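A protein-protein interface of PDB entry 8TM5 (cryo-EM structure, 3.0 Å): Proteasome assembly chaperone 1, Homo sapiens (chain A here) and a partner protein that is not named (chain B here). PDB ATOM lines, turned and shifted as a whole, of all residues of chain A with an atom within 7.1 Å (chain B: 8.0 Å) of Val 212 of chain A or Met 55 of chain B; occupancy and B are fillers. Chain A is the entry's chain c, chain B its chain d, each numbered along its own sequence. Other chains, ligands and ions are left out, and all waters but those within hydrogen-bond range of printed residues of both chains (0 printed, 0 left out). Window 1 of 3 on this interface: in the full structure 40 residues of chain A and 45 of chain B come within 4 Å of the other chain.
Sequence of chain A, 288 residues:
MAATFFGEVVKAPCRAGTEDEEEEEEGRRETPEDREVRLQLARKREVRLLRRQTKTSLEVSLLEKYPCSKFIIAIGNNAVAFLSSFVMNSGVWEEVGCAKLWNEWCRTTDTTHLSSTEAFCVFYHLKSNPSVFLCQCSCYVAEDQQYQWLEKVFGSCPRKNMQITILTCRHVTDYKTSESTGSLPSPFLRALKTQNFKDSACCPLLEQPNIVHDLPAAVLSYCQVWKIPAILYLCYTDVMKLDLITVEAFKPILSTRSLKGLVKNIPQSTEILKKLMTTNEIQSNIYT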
ATOM      1  N   GLN A 146      -7.433   8.727 -18.199  1.00  0.00           N
ATOM      2  CA  GLN A 146      -8.801   8.226 -18.267  1.00  0.00           C
ATOM      3  C   GLN A 146      -9.403   8.427 -19.652  1.00  0.00           C
ATOM      4  O   GLN A 146      -9.980   7.495 -20.221  1.00  0.00           O
ATOM      5  CB  GLN A 146      -9.658   8.910 -17.203  1.00  0.00           C
ATOM      6  CG  GLN A 146      -9.466   8.337 -15.810  1.00  0.00           C
ATOM      7  CD  GLN A 146      -9.707   9.358 -14.721  1.00  0.00           C
ATOM      8  OE1 GLN A 146     -10.484  10.294 -14.893  1.00  0.00           O
ATOM      9  NE2 GLN A 146      -9.035   9.184 -13.590  1.00  0.00           N
ATOM     10  N   TYR A 147      -9.270   9.628 -20.216  1.00  0.00           N
ATOM     11  CA  TYR A 147      -9.768   9.851 -21.568  1.00  0.00           C
ATOM     12  C   TYR A 147      -8.976   9.047 -22.591  1.00  0.00           C
ATOM     13  O   TYR A 147      -9.538   8.611 -23.603  1.00  0.00           O
ATOM     14  CB  TYR A 147      -9.728  11.340 -21.904  1.00  0.00           C
ATOM     15  CG  TYR A 147     -10.859  12.122 -21.281  1.00  0.00           C
ATOM     16  CD1 TYR A 147     -12.116  12.143 -21.866  1.00  0.00           C
ATOM     17  CD2 TYR A 147     -10.674  12.833 -20.104  1.00  0.00           C
ATOM     18  CE1 TYR A 147     -13.156  12.853 -21.300  1.00  0.00           C
ATOM     19  CE2 TYR A 147     -11.708  13.546 -19.530  1.00  0.00           C
ATOM     20  CZ  TYR A 147     -12.946  13.553 -20.133  1.00  0.00           C
ATOM     21  OH  TYR A 147     -13.980  14.261 -19.567  1.00  0.00           O
ATOM     22  N   ARG A 170     -16.134   1.923  -3.261  1.00  0.00           N
ATOM     23  CA  ARG A 170     -15.766   3.154  -2.581  1.00  0.00           C
ATOM     24  C   ARG A 170     -15.794   2.912  -1.077  1.00  0.00           C
ATOM     25  O   ARG A 170     -16.208   1.851  -0.602  1.00  0.00           O
ATOM     26  CB  ARG A 170     -16.710   4.300  -2.964  1.00  0.00           C
ATOM     27  CG  ARG A 170     -16.572   4.796  -4.399  1.00  0.00           C
ATOM     28  CD  ARG A 170     -15.147   5.204  -4.739  1.00  0.00           C
ATOM     29  NE  ARG A 170     -15.073   5.866  -6.037  1.00  0.00           N
ATOM     30  CZ  ARG A 170     -14.085   5.721  -6.910  1.00  0.00           C
ATOM     31  NH1 ARG A 170     -13.041   4.948  -6.657  1.00  0.00           N
ATOM     32  NH2 ARG A 170     -14.144   6.371  -8.069  1.00  0.00           N
ATOM     33  N   LEU A 192     -25.862   4.950 -10.533  1.00  0.00           N
ATOM     34  CA  LEU A 192     -25.879   6.146 -11.368  1.00  0.00           C
ATOM     35  C   LEU A 192     -25.997   5.688 -12.813  1.00  0.00           C
ATOM     36  O   LEU A 192     -25.108   4.993 -13.315  1.00  0.00           O
ATOM     37  CB  LEU A 192     -24.613   6.987 -11.173  1.00  0.00           C
ATOM     38  CG  LEU A 192     -24.537   7.857  -9.916  1.00  0.00           C
ATOM     39  CD1 LEU A 192     -23.175   8.521  -9.822  1.00  0.00           C
ATOM     40  CD2 LEU A 192     -25.639   8.902  -9.912  1.00  0.00           C
ATOM     41  N   LEU A 206     -27.665   7.316  -6.111  1.00  0.00           N
ATOM     42  CA  LEU A 206     -26.745   8.120  -5.324  1.00  0.00           C
ATOM     43  C   LEU A 206     -27.357   9.478  -5.003  1.00  0.00           C
ATOM     44  O   LEU A 206     -28.091  10.061  -5.806  1.00  0.00           O
ATOM     45  CB  LEU A 206     -25.423   8.304  -6.070  1.00  0.00           C
ATOM     46  CG  LEU A 206     -24.269   8.893  -5.258  1.00  0.00           C
ATOM     47  CD1 LEU A 206     -23.892   7.979  -4.102  1.00  0.00           C
ATOM     48  CD2 LEU A 206     -23.068   9.149  -6.153  1.00  0.00           C
ATOM     49  N   PRO A 209     -25.494  15.629  -3.183  1.00  0.00           N
ATOM     50  CA  PRO A 209     -24.143  16.128  -2.885  1.00  0.00           C
ATOM     51  C   PRO A 209     -23.057  15.093  -3.108  1.00  0.00           C
ATOM     52  O   PRO A 209     -21.883  15.464  -3.223  1.00  0.00           O
ATOM     53  CB  PRO A 209     -24.235  16.540  -1.409  1.00  0.00           C
ATOM     54  CG  PRO A 209     -25.369  15.754  -0.863  1.00  0.00           C
ATOM     55  CD  PRO A 209     -26.351  15.613  -1.986  1.00  0.00           C
ATOM     56  N   ASN A 210     -23.409  13.812  -3.177  1.00  0.00           N
ATOM     57  CA  ASN A 210     -22.439  12.759  -3.452  1.00  0.00           C
ATOM     58  C   ASN A 210     -22.151  12.709  -4.947  1.00  0.00           C
ATOM     59  O   ASN A 210     -23.069  12.553  -5.759  1.00  0.00           O
ATOM     60  CB  ASN A 210     -22.968  11.418  -2.957  1.00  0.00           C
ATOM     61  CG  ASN A 210     -23.149  11.384  -1.459  1.00  0.00           C
ATOM     62  OD1 ASN A 210     -22.610  12.222  -0.739  1.00  0.00           O
ATOM     63  ND2 ASN A 210     -23.919  10.419  -0.978  1.00  0.00           N
ATOM     64  N   ILE A 211     -20.880  12.844  -5.311  1.00  0.00           N
ATOM     65  CA  ILE A 211     -20.438  12.732  -6.693  1.00  0.00           C
ATOM     66  C   ILE A 211     -19.277  11.751  -6.748  1.00  0.00           C
ATOM     67  O   ILE A 211     -18.629  11.459  -5.740  1.00  0.00           O
ATOM     68  CB  ILE A 211     -20.030  14.095  -7.286  1.00  0.00           C
ATOM     69  CG1 ILE A 211     -19.001  14.787  -6.391  1.00  0.00           C
ATOM     70  CG2 ILE A 211     -21.250  14.980  -7.461  1.00  0.00           C
ATOM     71  CD1 ILE A 211     -18.085  15.728  -7.138  1.00  0.00           C
ATOM     72  N   VAL A 212     -19.020  11.236  -7.947  1.00  0.00           N
ATOM     73  CA  VAL A 212     -17.953  10.272  -8.171  1.00  0.00           C
ATOM     74  C   VAL A 212     -17.032  10.811  -9.259  1.00  0.00           C
ATOM     75  O   VAL A 212     -17.387  11.712 -10.018  1.00  0.00           O
ATOM     76  CB  VAL A 212     -18.493   8.881  -8.548  1.00  0.00           C
ATOM     77  CG1 VAL A 212     -19.513   8.418  -7.526  1.00  0.00           C
ATOM     78  CG2 VAL A 212     -19.095   8.904  -9.936  1.00  0.00           C
ATOM     79  N   HIS A 213     -15.839  10.235  -9.327  1.00  0.00           N
ATOM     80  CA  HIS A 213     -14.803  10.688 -10.244  1.00  0.00           C
ATOM     81  C   HIS A 213     -13.998   9.469 -10.681  1.00  0.00           C
ATOM     82  O   HIS A 213     -14.415   8.325 -10.475  1.00  0.00           O
ATOM     83  CB  HIS A 213     -13.929  11.758  -9.582  1.00  0.00           C
ATOM     84  CG  HIS A 213     -13.263  11.297  -8.324  1.00  0.00           C
ATOM     85  ND1 HIS A 213     -12.007  10.733  -8.309  1.00  0.00           N
ATOM     86  CD2 HIS A 213     -13.682  11.316  -7.036  1.00  0.00           C
ATOM     87  CE1 HIS A 213     -11.678  10.425  -7.068  1.00  0.00           C
ATOM     88  NE2 HIS A 213     -12.678  10.767  -6.275  1.00  0.00           N
ATOM     89  N   ASP A 214     -12.843   9.717 -11.298  1.00  0.00           N
ATOM     90  CA  ASP A 214     -11.949   8.647 -11.727  1.00  0.00           C
ATOM     91  C   ASP A 214     -12.483   7.961 -12.978  1.00  0.00           C
ATOM     92  O   ASP A 214     -13.382   8.483 -13.646  1.00  0.00           O
ATOM     93  CB  ASP A 214     -11.754   7.626 -10.604  1.00  0.00           C
ATOM     94  N   PRO A 216     -14.448   5.260 -13.564  1.00  0.00           N
ATOM     95  CA  PRO A 216     -15.888   4.973 -13.687  1.00  0.00           C
ATOM     96  C   PRO A 216     -16.696   6.197 -14.072  1.00  0.00           C
ATOM     97  O   PRO A 216     -17.609   6.109 -14.906  1.00  0.00           O
ATOM     98  CB  PRO A 216     -16.265   4.458 -12.289  1.00  0.00           C
ATOM     99  CG  PRO A 216     -14.984   4.071 -11.643  1.00  0.00           C
ATOM    100  CD  PRO A 216     -13.930   4.949 -12.222  1.00  0.00           C
ATOM    101  N   ALA A 217     -16.366   7.350 -13.491  1.00  0.00           N
ATOM    102  CA  ALA A 217     -17.035   8.587 -13.869  1.00  0.00           C
ATOM    103  C   ALA A 217     -16.771   8.915 -15.330  1.00  0.00           C
ATOM    104  O   ALA A 217     -17.665   9.379 -16.043  1.00  0.00           O
ATOM    105  CB  ALA A 217     -16.574   9.730 -12.968  1.00  0.00           C
ATOM    106  N   ALA A 218     -15.542   8.680 -15.794  1.00  0.00           N
ATOM    107  CA  ALA A 218     -15.221   8.928 -17.194  1.00  0.00           C
ATOM    108  C   ALA A 218     -16.092   8.078 -18.108  1.00  0.00           C
ATOM    109  O   ALA A 218     -16.655   8.574 -19.089  1.00  0.00           O
ATOM    110  CB  ALA A 218     -13.741   8.643 -17.448  1.00  0.00           C
ATOM    111  N   LEU A 220     -19.022   6.617 -17.451  1.00  0.00           N
ATOM    112  CA  LEU A 220     -20.429   6.989 -17.388  1.00  0.00           C
ATOM    113  C   LEU A 220     -20.693   8.309 -18.100  1.00  0.00           C
ATOM    114  O   LEU A 220     -21.712   8.447 -18.783  1.00  0.00           O
ATOM    115  CB  LEU A 220     -20.894   7.059 -15.935  1.00  0.00           C
ATOM    116  CG  LEU A 220     -22.413   7.048 -15.754  1.00  0.00           C
ATOM    117  CD1 LEU A 220     -22.978   5.670 -16.052  1.00  0.00           C
ATOM    118  CD2 LEU A 220     -22.783   7.481 -14.348  1.00  0.00           C
ATOM    119  N   SER A 221     -19.793   9.284 -17.965  1.00  0.00           N
ATOM    120  CA  SER A 221     -19.950  10.547 -18.675  1.00  0.00           C
ATOM    121  C   SER A 221     -19.842  10.358 -20.182  1.00  0.00           C
ATOM    122  O   SER A 221     -20.586  10.984 -20.942  1.00  0.00           O
ATOM    123  CB  SER A 221     -18.907  11.553 -18.189  1.00  0.00           C
ATOM    124  OG  SER A 221     -17.602  11.148 -18.561  1.00  0.00           O
ATOM    125  N   LEU A 232     -23.686   2.820 -13.411  1.00  0.00           N
ATOM    126  CA  LEU A 232     -22.476   2.799 -12.598  1.00  0.00           C
ATOM    127  C   LEU A 232     -22.884   2.498 -11.164  1.00  0.00           C
ATOM    128  O   LEU A 232     -23.763   3.171 -10.614  1.00  0.00           O
ATOM    129  CB  LEU A 232     -21.736   4.134 -12.699  1.00  0.00           C
ATOM    130  CG  LEU A 232     -20.313   4.240 -12.146  1.00  0.00           C
ATOM    131  CD1 LEU A 232     -19.659   5.482 -12.722  1.00  0.00           C
ATOM    132  CD2 LEU A 232     -20.288   4.288 -10.640  1.00  0.00           C
ATOM    133  N   LEU A 234     -22.100   1.906  -7.066  1.00  0.00           N
ATOM    134  CA  LEU A 234     -21.261   2.457  -6.004  1.00  0.00           C
ATOM    135  C   LEU A 234     -21.333   1.526  -4.798  1.00  0.00           C
ATOM    136  O   LEU A 234     -22.211   1.654  -3.946  1.00  0.00           O
ATOM    137  CB  LEU A 234     -21.718   3.865  -5.629  1.00  0.00           C
ATOM    138  CG  LEU A 234     -21.063   5.057  -6.320  1.00  0.00           C
ATOM    139  CD1 LEU A 234     -19.554   5.036  -6.146  1.00  0.00           C
ATOM    140  CD2 LEU A 234     -21.455   5.074  -7.778  1.00  0.00           C
ATOM    141  N   TYR A 236     -20.177   1.009  -1.532  1.00  0.00           N
ATOM    142  CA  TYR A 236     -19.511   1.634  -0.400  1.00  0.00           C
ATOM    143  C   TYR A 236     -19.227   0.600   0.680  1.00  0.00           C
ATOM    144  O   TYR A 236     -20.064  -0.258   0.975  1.00  0.00           O
ATOM    145  CB  TYR A 236     -20.364   2.766   0.172  1.00  0.00           C
ATOM    146  CG  TYR A 236     -20.499   3.951  -0.752  1.00  0.00           C
ATOM    147  CD1 TYR A 236     -19.491   4.900  -0.842  1.00  0.00           C
ATOM    148  CD2 TYR A 236     -21.634   4.126  -1.527  1.00  0.00           C
ATOM    149  CE1 TYR A 236     -19.608   5.986  -1.683  1.00  0.00           C
ATOM    150  CE2 TYR A 236     -21.761   5.212  -2.369  1.00  0.00           C
ATOM    151  CZ  TYR A 236     -20.745   6.137  -2.444  1.00  0.00           C
ATOM    152  OH  TYR A 236     -20.865   7.220  -3.283  1.00  0.00           O
ATOM    153  N   LEU B  52     -11.184  18.621 -18.504  1.00  0.00           N
ATOM    154  CA  LEU B  52     -11.656  18.555 -17.130  1.00  0.00           C
ATOM    155  C   LEU B  52     -11.612  17.119 -16.620  1.00  0.00           C
ATOM    156  O   LEU B  52     -11.731  16.157 -17.382  1.00  0.00           O
ATOM    157  CB  LEU B  52     -13.082  19.099 -17.025  1.00  0.00           C
ATOM    158  CG  LEU B  52     -13.239  20.610 -16.831  1.00  0.00           C
ATOM    159  CD1 LEU B  52     -12.718  21.049 -15.473  1.00  0.00           C
ATOM    160  CD2 LEU B  52     -12.527  21.366 -17.938  1.00  0.00           C
ATOM    161  N   VAL B  53     -11.433  16.984 -15.314  1.00  0.00           N
ATOM    162  CA  VAL B  53     -11.466  15.664 -14.682  1.00  0.00           C
ATOM    163  C   VAL B  53     -12.912  15.175 -14.650  1.00  0.00           C
ATOM    164  O   VAL B  53     -13.778  15.873 -14.100  1.00  0.00           O
ATOM    165  CB  VAL B  53     -10.872  15.725 -13.280  1.00  0.00           C
ATOM    166  CG1 VAL B  53     -10.966  14.368 -12.599  1.00  0.00           C
ATOM    167  CG2 VAL B  53      -9.425  16.174 -13.351  1.00  0.00           C
ATOM    168  N   PRO B  54     -13.213  14.005 -15.212  1.00  0.00           N
ATOM    169  CA  PRO B  54     -14.616  13.586 -15.331  1.00  0.00           C
ATOM    170  C   PRO B  54     -15.249  13.323 -13.972  1.00  0.00           C
ATOM    171  O   PRO B  54     -14.602  12.817 -13.053  1.00  0.00           O
ATOM    172  CB  PRO B  54     -14.536  12.309 -16.175  1.00  0.00           C
ATOM    173  CG  PRO B  54     -13.166  11.789 -15.955  1.00  0.00           C
ATOM    174  CD  PRO B  54     -12.281  12.970 -15.694  1.00  0.00           C
ATOM    175  N   MET B  55     -16.527  13.676 -13.857  1.00  0.00           N
ATOM    176  CA  MET B  55     -17.342  13.362 -12.696  1.00  0.00           C
ATOM    177  C   MET B  55     -18.766  13.106 -13.167  1.00  0.00           C
ATOM    178  O   MET B  55     -19.156  13.509 -14.266  1.00  0.00           O
ATOM    179  CB  MET B  55     -17.334  14.494 -11.659  1.00  0.00           C
ATOM    180  CG  MET B  55     -17.854  15.821 -12.185  1.00  0.00           C
ATOM    181  SD  MET B  55     -19.112  16.555 -11.122  1.00  0.00           S
ATOM    182  CE  MET B  55     -20.540  15.562 -11.550  1.00  0.00           C
ATOM    183  N   VAL B  56     -19.546  12.430 -12.329  1.00  0.00           N
ATOM    184  CA  VAL B  56     -20.945  12.156 -12.637  1.00  0.00           C
ATOM    185  C   VAL B  56     -21.732  12.115 -11.336  1.00  0.00           C
ATOM    186  O   VAL B  56     -21.302  11.494 -10.359  1.00  0.00           O
ATOM    187  CB  VAL B  56     -21.119  10.838 -13.416  1.00  0.00           C
ATOM    188  CG1 VAL B  56     -20.630  10.997 -14.847  1.00  0.00           C
ATOM    189  CG2 VAL B  56     -20.398   9.696 -12.721  1.00  0.00           C
ATOM    190  N   GLY B  57     -22.883  12.780 -11.326  1.00  0.00           N
ATOM    191  CA  GLY B  57     -23.798  12.778 -10.200  1.00  0.00           C
ATOM    192  C   GLY B  57     -25.230  12.809 -10.697  1.00  0.00           C
ATOM    193  O   GLY B  57     -25.624  12.051 -11.580  1.00  0.00           O
ATOM    194  N   ASN B  58     -26.016  13.704 -10.111  1.00  0.00           N
ATOM    195  CA  ASN B  58     -27.360  14.004 -10.578  1.00  0.00           C
ATOM    196  C   ASN B  58     -27.503  15.511 -10.735  1.00  0.00           C
ATOM    197  O   ASN B  58     -26.642  16.286 -10.315  1.00  0.00           O
ATOM    198  CB  ASN B  58     -28.423  13.454  -9.620  1.00  0.00           C
ATOM    199  CG  ASN B  58     -28.507  11.941  -9.650  1.00  0.00           C
ATOM    200  OD1 ASN B  58     -28.551  11.334 -10.718  1.00  0.00           O
ATOM    201  ND2 ASN B  58     -28.540  11.327  -8.475  1.00  0.00           N
ATOM    202  N   PRO B  60     -27.734  19.092 -10.306  1.00  0.00           N
ATOM    203  CA  PRO B  60     -27.581  19.846  -9.050  1.00  0.00           C
ATOM    204  C   PRO B  60     -28.805  20.661  -8.678  1.00  0.00           C
ATOM    205  O   PRO B  60     -29.061  20.881  -7.488  1.00  0.00           O
ATOM    206  CB  PRO B  60     -26.364  20.744  -9.317  1.00  0.00           C
ATOM    207  CG  PRO B  60     -25.698  20.192 -10.523  1.00  0.00           C
ATOM    208  CD  PRO B  60     -26.736  19.480 -11.316  1.00  0.00           C
ATOM    209  N   LEU B  71     -28.805  12.485 -14.897  1.00  0.00           N
ATOM    210  CA  LEU B  71     -27.365  12.379 -14.717  1.00  0.00           C
ATOM    211  C   LEU B  71     -26.668  13.642 -15.206  1.00  0.00           C
ATOM    212  O   LEU B  71     -26.993  14.174 -16.271  1.00  0.00           O
ATOM    213  CB  LEU B  71     -26.838  11.154 -15.466  1.00  0.00           C
ATOM    214  CG  LEU B  71     -25.324  10.939 -15.461  1.00  0.00           C
ATOM    215  CD1 LEU B  71     -24.846  10.500 -14.092  1.00  0.00           C
ATOM    216  CD2 LEU B  71     -24.937   9.913 -16.506  1.00  0.00           C
ATOM    217  N   SER B  72     -25.711  14.116 -14.418  1.00  0.00           N
ATOM    218  CA  SER B  72     -24.906  15.280 -14.752  1.00  0.00           C
ATOM    219  C   SER B  72     -23.445  14.877 -14.911  1.00  0.00           C
ATOM    220  O   SER B  72     -23.011  13.827 -14.431  1.00  0.00           O
ATOM    221  CB  SER B  72     -25.036  16.356 -13.673  1.00  0.00           C
ATOM    222  OG  SER B  72     -24.156  17.436 -13.926  1.00  0.00           O
ATOM    223  N   ILE B  73     -22.686  15.728 -15.599  1.00  0.00           N
ATOM    224  CA  ILE B  73     -21.264  15.508 -15.820  1.00  0.00           C
ATOM    225  C   ILE B  73     -20.513  16.793 -15.492  1.00  0.00           C
ATOM    226  O   ILE B  73     -21.101  17.812 -15.131  1.00  0.00           O
ATOM    227  CB  ILE B  73     -20.956  15.034 -17.258  1.00  0.00           C
ATOM    228  CG1 ILE B  73     -21.036  16.188 -18.260  1.00  0.00           C
ATOM    229  CG2 ILE B  73     -21.917  13.928 -17.662  1.00  0.00           C
ATOM    230  CD1 ILE B  73     -20.634  15.785 -19.658  1.00  0.00           C
ATOM    231  N   ASN B  74     -19.188  16.726 -15.624  1.00  0.00           N
ATOM    232  CA  ASN B  74     -18.320  17.829 -15.226  1.00  0.00           C
ATOM    233  C   ASN B  74     -18.673  19.116 -15.958  1.00  0.00           C
ATOM    234  O   ASN B  74     -18.846  20.165 -15.328  1.00  0.00           O
ATOM    235  CB  ASN B  74     -16.854  17.469 -15.479  1.00  0.00           C
ATOM    236  CG  ASN B  74     -16.620  16.927 -16.872  1.00  0.00           C
ATOM    237  OD1 ASN B  74     -17.561  16.735 -17.642  1.00  0.00           O
ATOM    238  ND2 ASN B  74     -15.360  16.675 -17.206  1.00  0.00           N
ATOM    239  N   ALA B  75     -18.782  19.052 -17.282  1.00  0.00           N
ATOM    240  CA  ALA B  75     -19.060  20.221 -18.115  1.00  0.00           C
ATOM    241  C   ALA B  75     -20.429  20.037 -18.760  1.00  0.00           C
ATOM    242  O   ALA B  75     -20.615  19.156 -19.604  1.00  0.00           O
ATOM    243  CB  ALA B  75     -17.970  20.409 -19.165  1.00  0.00           C
ATOM    244  N   GLU B  76     -21.383  20.876 -18.365  1.00  0.00           N
ATOM    245  CA  GLU B  76     -22.733  20.858 -18.911  1.00  0.00           C
ATOM    246  C   GLU B  76     -23.108  22.269 -19.336  1.00  0.00           C
ATOM    247  O   GLU B  76     -22.765  23.238 -18.652  1.00  0.00           O
ATOM    248  CB  GLU B  76     -23.735  20.322 -17.887  1.00  0.00           C
ATOM    249  CG  GLU B  76     -23.569  18.843 -17.584  1.00  0.00           C
ATOM    250  CD  GLU B  76     -24.820  18.221 -17.001  1.00  0.00           C
ATOM    251  OE1 GLU B  76     -25.324  18.739 -15.981  1.00  0.00           O
ATOM    252  OE2 GLU B  76     -25.301  17.214 -17.560  1.00  0.00           O
ATOM    253  N   GLN B  89     -21.237  25.192 -17.320  1.00  0.00           N
ATOM    254  CA  GLN B  89     -21.064  24.880 -15.898  1.00  0.00           C
ATOM    255  C   GLN B  89     -19.955  23.841 -15.752  1.00  0.00           C
ATOM    256  O   GLN B  89     -20.181  22.642 -15.934  1.00  0.00           O
ATOM    257  CB  GLN B  89     -22.372  24.394 -15.287  1.00  0.00           C
ATOM    258  CG  GLN B  89     -22.283  24.085 -13.801  1.00  0.00           C
ATOM    259  CD  GLN B  89     -21.812  25.271 -12.985  1.00  0.00           C
ATOM    260  OE1 GLN B  89     -22.581  26.187 -12.699  1.00  0.00           O
ATOM    261  NE2 GLN B  89     -20.540  25.259 -12.607  1.00  0.00           N
ATOM    262  N   LEU B  90     -18.756  24.312 -15.422  1.00  0.00           N
ATOM    263  CA  LEU B  90     -17.670  23.409 -15.069  1.00  0.00           C
ATOM    264  C   LEU B  90     -17.794  23.002 -13.607  1.00  0.00           C
ATOM    265  O   LEU B  90     -17.874  23.854 -12.718  1.00  0.00           O
ATOM    266  CB  LEU B  90     -16.322  24.082 -15.315  1.00  0.00           C
ATOM    267  CG  LEU B  90     -16.015  24.508 -16.751  1.00  0.00           C
ATOM    268  CD1 LEU B  90     -14.587  25.006 -16.852  1.00  0.00           C
ATOM    269  CD2 LEU B  90     -16.250  23.363 -17.723  1.00  0.00           C
ATOM    270  N   ARG B  91     -17.808  21.697 -13.358  1.00  0.00           N
ATOM    271  CA  ARG B  91     -17.939  21.155 -12.012  1.00  0.00           C
ATOM    272  C   ARG B  91     -16.767  20.244 -11.683  1.00  0.00           C
ATOM    273  O   ARG B  91     -16.923  19.218 -11.014  1.00  0.00           O
ATOM    274  CB  ARG B  91     -19.260  20.407 -11.854  1.00  0.00           C
ATOM    275  CG  ARG B  91     -20.491  21.245 -12.153  1.00  0.00           C
ATOM    276  CD  ARG B  91     -21.741  20.615 -11.568  1.00  0.00           C
ATOM    277  NE  ARG B  91     -22.946  21.076 -12.248  1.00  0.00           N
ATOM    278  CZ  ARG B  91     -23.325  20.670 -13.451  1.00  0.00           C
ATOM    279  NH1 ARG B  91     -22.611  19.796 -14.141  1.00  0.00           N
ATOM    280  NH2 ARG B  91     -24.446  21.154 -13.976  1.00  0.00           N
ATOM    281  N   SER B  92     -15.570  20.603 -12.142  1.00  0.00           N
ATOM    282  CA  SER B  92     -14.395  19.779 -11.899  1.00  0.00           C
ATOM    283  C   SER B  92     -13.130  20.617 -11.978  1.00  0.00           C
ATOM    284  O   SER B  92     -13.110  21.714 -12.539  1.00  0.00           O
ATOM    285  CB  SER B  92     -14.296  18.628 -12.902  1.00  0.00           C
ATOM    286  OG  SER B  92     -15.194  17.589 -12.572  1.00  0.00           O
ATOM    287  N   ILE B  93     -12.066  20.063 -11.402  1.00  0.00           N
ATOM    288  CA  ILE B  93     -10.719  20.601 -11.525  1.00  0.00           C
ATOM    289  C   ILE B  93     -10.240  20.442 -12.961  1.00  0.00           C
ATOM    290  O   ILE B  93     -10.821  19.678 -13.740  1.00  0.00           O
ATOM    291  CB  ILE B  93      -9.772  19.904 -10.530  1.00  0.00           C
ATOM    292  CG1 ILE B  93      -9.383  18.504 -11.041  1.00  0.00           C
ATOM    293  CG2 ILE B  93     -10.409  19.836  -9.146  1.00  0.00           C
ATOM    294  CD1 ILE B  93      -8.210  17.911 -10.351  1.00  0.00           C
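The backbone carbonyl oxygen (O) of Asn 74 of chain B is in hydrogen-bond range of the backbone NH (N) of Arg 91 of chain B (2.7 Å).
The backbone carbonyl oxygen (O) of His 213 of chain A lies within hydrogen-bond range of the guanidinium group (NH2) of Arg 170 of chain A (3.1 Å).
The backbone carbonyl oxygen (O) of Met 55 of chain B sits at hydrogen-bond distance from the backbone NH (N) of Asn 74 of chain B (3.5 Å).
The guanidinium group (NH1) of Arg 91 of chain B lies within hydrogen-bond range of the backbone carbonyl oxygen (O) of Ile 73 of chain B (2.7 Å).
The backbone carbonyl oxygen (O) of Ala 217 of chain A lies within hydrogen-bond range of the side-chain hydroxyl (OG) of Ser 221 of chain A, 3.1 Å away.
The backbone NH of Leu 232 of chain A is in hydrogen-bond range of the backbone carbonyl oxygen of Leu 192 of chain A (2.6 Å).
Of the 19 printed residues of chain B, 9 touch a printed residue of chain A.
Printed residues of chain B that touch a printed residue of chain A: Leu 52, Pro 54, Met 55, Val 56, Gly 57, Asn 58, Leu 71, Ile 73 and Asn 74.
Hydrophobic or aromatic side chains of chain B within 4 Å of the printed part of chain A: Pro 54, Met 55, Val 56, Leu 71 and Ile 73.
Hydrophobic or aromatic side chains of chain A within 4 Å of the printed part of chain B: Tyr 147, Leu 192, Val 212, His 213, Ala 217, Ala 218 and Leu 220.
Among the printed residues, pairs that only touch across the chains: Gln 146 of chain A with Pro 54 of chain B, Tyr 147 of chain A with Leu 52 of chain B, Tyr 147 of chain A with Pro 54 of chain B, Tyr 147 of chain A with Asn 74 of chain B, Leu 192 of chain A with Val 56 of chain B, Leu 192 of chain A with Gly 57 of chain B, Leu 192 of chain A with Asn 58 of chain B, Ile 211 of chain A with Val 56 of chain B, Val 212 of chain A with Met 55 of chain B, His 213 of chain A with Pro 54 of chain B, Asp 214 of chain A with Pro 54 of chain B, Ala 217 of chain A with Pro 54 of chain B, Ala 217 of chain A with Met 55 of chain B, Ala 217 of chain A with Val 56 of chain B, Ala 218 of chain A with Pro 54 of chain B, Leu 220 of chain A with Val 56 of chain B, Leu 220 of chain A with Leu 71 of chain B, Ser 221 of chain A with Val 56 of chain B and Ser 221 of chain A with Ile 73 of chain B.
Of the printed residues of chain B, Gln 146 of chain A touches Pro 54 (3.2 Å).
Val 212 of chain A touches two residues of chain B.
Of the printed residues of chain A, Leu 52 of chain B touches Tyr 147 (3.4 Å).
Met 55 of chain B touches just these residues of chain A: Val 212 (3.1 Å) and Ala 217 (3.7 Å).
Of the printed residues of chain A, Asn 58 of chain B touches Leu 192 and Leu 206.
Of the printed residues of chain A, Ile 73 of chain B touches Ser 221 (3.9 Å).
The nearest residue of chain A that does not touch Met 55 of chain B is Ile 211 of chain A (4.2 Å).
The side-chain amide nitrogen (ND2) of Asn 58 of chain B lies within hydrogen-bond range of the backbone carbonyl oxygen (O) of Leu 206 of chain A.
The backbone carbonyl oxygen (O) of Val 212 of chain A sits at hydrogen-bond distance from the backbone NH (N) of Val 56 of chain B (3.2 Å).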
